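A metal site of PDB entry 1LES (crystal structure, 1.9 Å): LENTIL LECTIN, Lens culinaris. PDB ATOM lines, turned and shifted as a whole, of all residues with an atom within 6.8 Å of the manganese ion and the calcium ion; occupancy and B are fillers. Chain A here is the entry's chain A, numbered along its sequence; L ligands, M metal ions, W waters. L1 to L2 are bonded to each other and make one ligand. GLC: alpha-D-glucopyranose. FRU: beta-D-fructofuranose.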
ATOM      1  N   ASP A  81       2.787  10.999 -26.287  1.00  0.00           N
ATOM      2  CA  ASP A  81       3.518  11.659 -25.201  1.00  0.00           C
ATOM      3  C   ASP A  81       3.432  10.918 -23.876  1.00  0.00           C
ATOM      4  O   ASP A  81       4.259  11.131 -22.989  1.00  0.00           O
ATOM      5  CB  ASP A  81       2.994  13.067 -25.010  1.00  0.00           C
ATOM      6  CG  ASP A  81       3.806  14.081 -25.793  1.00  0.00           C
ATOM      7  OD1 ASP A  81       4.927  14.456 -25.333  1.00  0.00           O
ATOM      8  OD2 ASP A  81       3.322  14.490 -26.852  1.00  0.00           O
ATOM      9  N   GLY A  98       0.036  17.551 -25.808  1.00  0.00           N
ATOM     10  CA  GLY A  98       1.472  17.342 -25.975  1.00  0.00           C
ATOM     11  C   GLY A  98       2.166  16.882 -24.700  1.00  0.00           C
ATOM     12  O   GLY A  98       1.608  16.073 -23.936  1.00  0.00           O
ATOM     13  N   GLY A  99       3.324  17.421 -24.388  1.00  0.00           N
ATOM     14  CA  GLY A  99       4.001  16.943 -23.209  1.00  0.00           C
ATOM     15  C   GLY A  99       3.264  17.331 -21.913  1.00  0.00           C
ATOM     16  O   GLY A  99       3.698  16.915 -20.841  1.00  0.00           O
ATOM     17  N   TYR A 100       2.227  18.159 -21.963  1.00  0.00           N
ATOM     18  CA  TYR A 100       1.534  18.493 -20.715  1.00  0.00           C
ATOM     19  C   TYR A 100       0.495  17.448 -20.332  1.00  0.00           C
ATOM     20  O   TYR A 100      -0.207  17.570 -19.329  1.00  0.00           O
ATOM     21  CB  TYR A 100       0.909  19.865 -20.776  1.00  0.00           C
ATOM     22  CG  TYR A 100       1.937  20.935 -20.738  1.00  0.00           C
ATOM     23  CD1 TYR A 100       2.392  21.457 -19.543  1.00  0.00           C
ATOM     24  CD2 TYR A 100       2.453  21.427 -21.922  1.00  0.00           C
ATOM     25  CE1 TYR A 100       3.343  22.460 -19.527  1.00  0.00           C
ATOM     26  CE2 TYR A 100       3.403  22.428 -21.930  1.00  0.00           C
ATOM     27  CZ  TYR A 100       3.832  22.934 -20.741  1.00  0.00           C
ATOM     28  OH  TYR A 100       4.779  23.907 -20.820  1.00  0.00           O
ATOM     29  N   LEU A 101       0.384  16.442 -21.169  1.00  0.00           N
ATOM     30  CA  LEU A 101      -0.454  15.301 -20.929  1.00  0.00           C
ATOM     31  C   LEU A 101      -1.963  15.568 -20.745  1.00  0.00           C
ATOM     32  O   LEU A 101      -2.677  14.670 -20.274  1.00  0.00           O
ATOM     33  CB  LEU A 101       0.141  14.487 -19.763  1.00  0.00           C
ATOM     34  CG  LEU A 101       1.599  14.009 -19.997  1.00  0.00           C
ATOM     35  CD1 LEU A 101       2.168  13.331 -18.783  1.00  0.00           C
ATOM     36  CD2 LEU A 101       1.658  13.077 -21.144  1.00  0.00           C
ATOM     37  N   GLU A 119       1.953   9.835 -13.908  1.00  0.00           N
ATOM     38  CA  GLU A 119       2.254   9.763 -15.349  1.00  0.00           C
ATOM     39  C   GLU A 119       3.100   8.602 -15.826  1.00  0.00           C
ATOM     40  O   GLU A 119       3.889   8.045 -15.076  1.00  0.00           O
ATOM     41  CB  GLU A 119       2.888  11.059 -15.825  1.00  0.00           C
ATOM     42  CG  GLU A 119       4.131  11.361 -15.085  1.00  0.00           C
ATOM     43  CD  GLU A 119       4.907  12.511 -15.692  1.00  0.00           C
ATOM     44  OE1 GLU A 119       4.398  13.648 -15.833  1.00  0.00           O
ATOM     45  OE2 GLU A 119       6.098  12.256 -15.997  1.00  0.00           O
ATOM     46  N   ASP A 121       5.202   8.593 -18.725  1.00  0.00           N
ATOM     47  CA  ASP A 121       5.722   9.540 -19.716  1.00  0.00           C
ATOM     48  C   ASP A 121       6.677   8.859 -20.722  1.00  0.00           C
ATOM     49  O   ASP A 121       7.746   8.354 -20.354  1.00  0.00           O
ATOM     50  CB  ASP A 121       6.424  10.645 -18.913  1.00  0.00           C
ATOM     51  CG  ASP A 121       6.822  11.854 -19.747  1.00  0.00           C
ATOM     52  OD1 ASP A 121       6.842  11.775 -20.994  1.00  0.00           O
ATOM     53  OD2 ASP A 121       7.069  12.902 -19.115  1.00  0.00           O
ATOM     54  N   THR A 122       6.343   8.896 -22.002  1.00  0.00           N
ATOM     55  CA  THR A 122       7.161   8.227 -22.987  1.00  0.00           C
ATOM     56  C   THR A 122       8.093   9.149 -23.829  1.00  0.00           C
ATOM     57  O   THR A 122       8.795   8.649 -24.699  1.00  0.00           O
ATOM     58  CB  THR A 122       6.273   7.511 -23.970  1.00  0.00           C
ATOM     59  OG1 THR A 122       5.342   8.455 -24.485  1.00  0.00           O
ATOM     60  CG2 THR A 122       5.559   6.293 -23.318  1.00  0.00           C
ATOM     61  N   PHE A 123       8.096  10.472 -23.579  1.00  0.00           N
ATOM     62  CA  PHE A 123       8.878  11.409 -24.403  1.00  0.00           C
ATOM     63  C   PHE A 123       9.602  12.432 -23.587  1.00  0.00           C
ATOM     64  O   PHE A 123       9.018  13.069 -22.699  1.00  0.00           O
ATOM     65  CB  PHE A 123       7.960  12.113 -25.397  1.00  0.00           C
ATOM     66  CG  PHE A 123       8.661  13.093 -26.280  1.00  0.00           C
ATOM     67  CD1 PHE A 123       8.831  14.442 -25.868  1.00  0.00           C
ATOM     68  CD2 PHE A 123       9.179  12.685 -27.522  1.00  0.00           C
ATOM     69  CE1 PHE A 123       9.507  15.382 -26.655  1.00  0.00           C
ATOM     70  CE2 PHE A 123       9.847  13.609 -28.324  1.00  0.00           C
ATOM     71  CZ  PHE A 123      10.003  14.969 -27.875  1.00  0.00           C
ATOM     72  N   TYR A 124      10.895  12.614 -23.897  1.00  0.00           N
ATOM     73  CA  TYR A 124      11.701  13.538 -23.108  1.00  0.00           C
ATOM     74  C   TYR A 124      11.508  14.964 -23.439  1.00  0.00           C
ATOM     75  O   TYR A 124      11.838  15.373 -24.555  1.00  0.00           O
ATOM     76  CB  TYR A 124      13.189  13.178 -23.234  1.00  0.00           C
ATOM     77  CG  TYR A 124      14.137  14.230 -22.655  1.00  0.00           C
ATOM     78  CD1 TYR A 124      14.218  14.447 -21.294  1.00  0.00           C
ATOM     79  CD2 TYR A 124      14.968  14.982 -23.488  1.00  0.00           C
ATOM     80  CE1 TYR A 124      15.106  15.400 -20.772  1.00  0.00           C
ATOM     81  CE2 TYR A 124      15.841  15.928 -22.973  1.00  0.00           C
ATOM     82  CZ  TYR A 124      15.905  16.120 -21.625  1.00  0.00           C
ATOM     83  OH  TYR A 124      16.721  17.077 -21.086  1.00  0.00           O
ATOM     84  N   ASN A 125      10.886  15.743 -22.543  1.00  0.00           N
ATOM     85  CA  ASN A 125      10.673  17.200 -22.740  1.00  0.00           C
ATOM     86  C   ASN A 125      11.796  17.861 -21.937  1.00  0.00           C
ATOM     87  O   ASN A 125      11.782  17.911 -20.704  1.00  0.00           O
ATOM     88  CB  ASN A 125       9.290  17.703 -22.243  1.00  0.00           C
ATOM     89  CG  ASN A 125       8.131  17.041 -22.964  1.00  0.00           C
ATOM     90  OD1 ASN A 125       7.644  15.961 -22.553  1.00  0.00           O
ATOM     91  ND2 ASN A 125       7.738  17.617 -24.114  1.00  0.00           N
ATOM     92  N   TRP A 128      11.674  20.081 -18.616  1.00  0.00           N
ATOM     93  CA  TRP A 128      11.323  19.630 -17.249  1.00  0.00           C
ATOM     94  C   TRP A 128      11.523  18.161 -16.952  1.00  0.00           C
ATOM     95  O   TRP A 128      11.533  17.769 -15.777  1.00  0.00           O
ATOM     96  CB  TRP A 128       9.836  19.976 -16.872  1.00  0.00           C
ATOM     97  CG  TRP A 128       8.765  19.349 -17.849  1.00  0.00           C
ATOM     98  CD1 TRP A 128       8.384  18.014 -17.914  1.00  0.00           C
ATOM     99  CD2 TRP A 128       8.057  20.006 -18.920  1.00  0.00           C
ATOM    100  NE1 TRP A 128       7.526  17.826 -18.983  1.00  0.00           N
ATOM    101  CE2 TRP A 128       7.301  19.027 -19.602  1.00  0.00           C
ATOM    102  CE3 TRP A 128       7.994  21.341 -19.377  1.00  0.00           C
ATOM    103  CZ2 TRP A 128       6.495  19.323 -20.699  1.00  0.00           C
ATOM    104  CZ3 TRP A 128       7.177  21.627 -20.473  1.00  0.00           C
ATOM    105  CH2 TRP A 128       6.447  20.617 -21.108  1.00  0.00           C
ATOM    106  N   ASP A 129      11.601  17.321 -17.972  1.00  0.00           N
ATOM    107  CA  ASP A 129      11.742  15.900 -17.695  1.00  0.00           C
ATOM    108  C   ASP A 129      13.105  15.520 -17.133  1.00  0.00           C
ATOM    109  O   ASP A 129      14.081  16.240 -17.326  1.00  0.00           O
ATOM    110  CB  ASP A 129      11.413  15.137 -18.954  1.00  0.00           C
ATOM    111  CG  ASP A 129       9.919  14.926 -19.120  1.00  0.00           C
ATOM    112  OD1 ASP A 129       9.254  14.916 -18.061  1.00  0.00           O
ATOM    113  OD2 ASP A 129       9.419  14.739 -20.243  1.00  0.00           O
ATOM    114  N   PRO A 130      13.203  14.406 -16.405  1.00  0.00           N
ATOM    115  CA  PRO A 130      14.501  14.012 -15.836  1.00  0.00           C
ATOM    116  C   PRO A 130      15.636  13.906 -16.880  1.00  0.00           C
ATOM    117  O   PRO A 130      15.462  13.289 -17.944  1.00  0.00           O
ATOM    118  CB  PRO A 130      14.186  12.690 -15.111  1.00  0.00           C
ATOM    119  CG  PRO A 130      12.949  12.186 -15.794  1.00  0.00           C
ATOM    120  CD  PRO A 130      12.157  13.418 -16.091  1.00  0.00           C
ATOM    121  N   HIS A 136       9.704   7.318 -18.130  1.00  0.00           N
ATOM    122  CA  HIS A 136       9.588   7.207 -16.700  1.00  0.00           C
ATOM    123  C   HIS A 136       8.159   7.280 -16.178  1.00  0.00           C
ATOM    124  O   HIS A 136       7.271   7.854 -16.815  1.00  0.00           O
ATOM    125  CB  HIS A 136      10.341   8.408 -16.069  1.00  0.00           C
ATOM    126  CG  HIS A 136       9.929   9.750 -16.619  1.00  0.00           C
ATOM    127  ND1 HIS A 136      10.378  10.233 -17.844  1.00  0.00           N
ATOM    128  CD2 HIS A 136       9.114  10.708 -16.125  1.00  0.00           C
ATOM    129  CE1 HIS A 136       9.862  11.428 -18.055  1.00  0.00           C
ATOM    130  NE2 HIS A 136       9.086  11.744 -17.025  1.00  0.00           N
ATOM    131  N   ILE A 137       8.014   6.803 -14.940  1.00  0.00           N
ATOM    132  CA  ILE A 137       6.764   6.851 -14.175  1.00  0.00           C
ATOM    133  C   ILE A 137       7.007   8.034 -13.226  1.00  0.00           C
ATOM    134  O   ILE A 137       8.077   8.158 -12.673  1.00  0.00           O
ATOM    135  CB  ILE A 137       6.611   5.615 -13.333  1.00  0.00           C
ATOM    136  CG1 ILE A 137       6.478   4.409 -14.231  1.00  0.00           C
ATOM    137  CG2 ILE A 137       5.398   5.780 -12.427  1.00  0.00           C
ATOM    138  CD1 ILE A 137       6.594   3.112 -13.444  1.00  0.00           C
ATOM    139  N   GLY A 138       6.029   8.905 -12.996  1.00  0.00           N
ATOM    140  CA  GLY A 138       6.269  10.028 -12.120  1.00  0.00           C
ATOM    141  C   GLY A 138       5.000  10.412 -11.359  1.00  0.00           C
ATOM    142  O   GLY A 138       3.899  10.032 -11.783  1.00  0.00           O
ATOM    143  N   ASP A 140       2.951  13.540 -10.152  1.00  0.00           N
ATOM    144  CA  ASP A 140       2.843  14.961 -10.411  1.00  0.00           C
ATOM    145  C   ASP A 140       1.828  15.625  -9.452  1.00  0.00           C
ATOM    146  O   ASP A 140       0.699  15.174  -9.388  1.00  0.00           O
ATOM    147  CB  ASP A 140       2.284  15.190 -11.812  1.00  0.00           C
ATOM    148  CG  ASP A 140       3.151  14.607 -12.910  1.00  0.00           C
ATOM    149  OD1 ASP A 140       4.304  14.255 -12.647  1.00  0.00           O
ATOM    150  OD2 ASP A 140       2.679  14.503 -14.038  1.00  0.00           O
ATOM    151  N   ILE A 144       3.586  19.797 -14.196  1.00  0.00           N
ATOM    152  CA  ILE A 144       4.037  18.692 -15.100  1.00  0.00           C
ATOM    153  C   ILE A 144       5.457  18.206 -14.714  1.00  0.00           C
ATOM    154  O   ILE A 144       5.934  17.146 -15.147  1.00  0.00           O
ATOM    155  CB  ILE A 144       3.974  19.119 -16.598  1.00  0.00           C
ATOM    156  CG1 ILE A 144       4.150  17.908 -17.515  1.00  0.00           C
ATOM    157  CG2 ILE A 144       5.005  20.222 -16.866  1.00  0.00           C
ATOM    158  CD1 ILE A 144       3.043  16.836 -17.362  1.00  0.00           C
ATOM    159  N   LYS A 145       6.104  18.960 -13.835  1.00  0.00           N
ATOM    160  CA  LYS A 145       7.446  18.568 -13.352  1.00  0.00           C
ATOM    161  C   LYS A 145       7.271  17.643 -12.167  1.00  0.00           C
ATOM    162  O   LYS A 145       7.045  18.147 -11.073  1.00  0.00           O
ATOM    163  CB  LYS A 145       8.159  19.817 -12.873  1.00  0.00           C
ATOM    164  CG  LYS A 145       9.534  19.877 -13.356  1.00  0.00           C
ATOM    165  CD  LYS A 145      10.478  19.610 -12.275  1.00  0.00           C
ATOM    166  CE  LYS A 145      11.147  20.913 -11.872  1.00  0.00           C
ATOM    167  NZ  LYS A 145      11.978  20.642 -10.643  1.00  0.00           N
ATOM    168  N   SER A 146       7.398  16.333 -12.325  1.00  0.00           N
ATOM    169  CA  SER A 146       7.186  15.404 -11.206  1.00  0.00           C
ATOM    170  C   SER A 146       7.943  15.648  -9.921  1.00  0.00           C
ATOM    171  O   SER A 146       9.061  16.137  -9.939  1.00  0.00           O
ATOM    172  CB  SER A 146       7.513  13.997 -11.654  1.00  0.00           C
ATOM    173  OG  SER A 146       6.964  13.785 -12.932  1.00  0.00           O
ATOM    174  N   THR A 149      10.428  10.467  -9.720  1.00  0.00           N
ATOM    175  CA  THR A 149      10.261   9.701 -10.974  1.00  0.00           C
ATOM    176  C   THR A 149      10.990   8.390 -10.884  1.00  0.00           C
ATOM    177  O   THR A 149      11.819   8.235 -10.046  1.00  0.00           O
ATOM    178  CB  THR A 149      10.898  10.424 -12.165  1.00  0.00           C
ATOM    179  OG1 THR A 149      12.233  10.796 -11.815  1.00  0.00           O
ATOM    180  CG2 THR A 149      10.155  11.703 -12.494  1.00  0.00           C
HETATM  181  C1  GLC L   1       6.054  18.735 -29.760  1.00  0.00           C
HETATM  182  C2  GLC L   1       5.043  19.201 -28.667  1.00  0.00           C
HETATM  183  C3  GLC L   1       5.423  18.695 -27.346  1.00  0.00           C
HETATM  184  C4  GLC L   1       5.401  17.217 -27.394  1.00  0.00           C
HETATM  185  C5  GLC L   1       6.380  16.631 -28.495  1.00  0.00           C
HETATM  186  C6  GLC L   1       6.289  15.095 -28.590  1.00  0.00           C
HETATM  187  O2  GLC L   1       5.067  20.593 -28.622  1.00  0.00           O
HETATM  188  O3  GLC L   1       4.470  19.145 -26.293  1.00  0.00           O
HETATM  189  O4  GLC L   1       5.845  16.805 -26.092  1.00  0.00           O
HETATM  190  O5  GLC L   1       5.978  17.318 -29.714  1.00  0.00           O
HETATM  191  O6  GLC L   1       5.106  14.747 -29.162  1.00  0.00           O
HETATM  192  C1  FRU L   2       7.738  21.124 -30.911  1.00  0.00           C
HETATM  193  C2  FRU L   2       8.233  19.798 -30.351  1.00  0.00           C
HETATM  194  C3  FRU L   2       9.587  20.037 -29.812  1.00  0.00           C
HETATM  195  C4  FRU L   2      10.025  18.580 -29.767  1.00  0.00           C
HETATM  196  C5  FRU L   2       9.685  18.064 -31.086  1.00  0.00           C
HETATM  197  C6  FRU L   2       9.554  16.604 -30.893  1.00  0.00           C
HETATM  198  O1  FRU L   2       8.494  21.502 -32.084  1.00  0.00           O
HETATM  199  O2  FRU L   2       7.350  19.174 -29.310  1.00  0.00           O
HETATM  200  O3  FRU L   2       9.567  20.437 -28.474  1.00  0.00           O
HETATM  201  O4  FRU L   2      11.456  18.465 -29.621  1.00  0.00           O
HETATM  202  O5  FRU L   2       8.491  18.794 -31.372  1.00  0.00           O
HETATM  203  O6  FRU L   2       9.372  16.064 -32.176  1.00  0.00           O
HETATM  204 MN    MN M   1       7.770  13.492 -17.147  1.00  0.00          MN
HETATM  205 CA    CA M   2       7.438  14.097 -21.301  1.00  0.00          CA
HETATM  206  O   HOH W   1       8.471  14.111 -15.387  1.00  0.00           O
HETATM  207  O   HOH W   2       6.212  15.125 -17.120  1.00  0.00           O
HETATM  208  O   HOH W   3       5.928  15.481 -19.972  1.00  0.00           O
HETATM  209  O   HOH W   4       5.728  13.619 -22.662  1.00  0.00           O
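The manganese ion is bound by water W1 (2.0 Å), the side-chain carboxylate of Asp 121 (2.2 Å), a ring nitrogen (NE2) of His 136 (2.2 Å), the side-chain carboxylate of Asp 129 (2.3 Å), water W2 (2.3 Å) and the side-chain carboxylate of Glu 119 (2.4 Å).
ND2 of Asn 125 is in hydrogen-bond range of O4 of GLC L1 (2.9 Å). The side-chain carboxylate (OD1) of Asp 81 sits at hydrogen-bond distance from an oxygen (O4) of GLC L1. An oxygen (O3) of GLC L1 lies within hydrogen-bond range of the backbone NH of Gly 99 (2.8 Å).
The calcium ion is bound by water W4, OD1 of Asn 125, OD2 of Asp 129, O of Phe 123, OD1 of Asp 121, water W3 and OD2 of Asp 121.
Within 4 Å of the calcium ion: Asp 121, Phe 123, Asn 125 and Asp 129. The nearest printed residue that does not touch the calcium ion is Trp 128 (4.4 Å).
Water W2 lies within hydrogen-bond range of OE1 of Glu 119 (2.7 Å) and O of Ile 144 (2.8 Å). Water W3 bridges O of Gly 99 (2.8 Å) and NE1 of Trp 128 (3.0 Å).
OE1 of Glu 119 lies close to OD2 of Asp 140 (2.6 Å). O of Gly 138 sits at hydrogen-bond distance from N of Glu 119 (2.9 Å).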
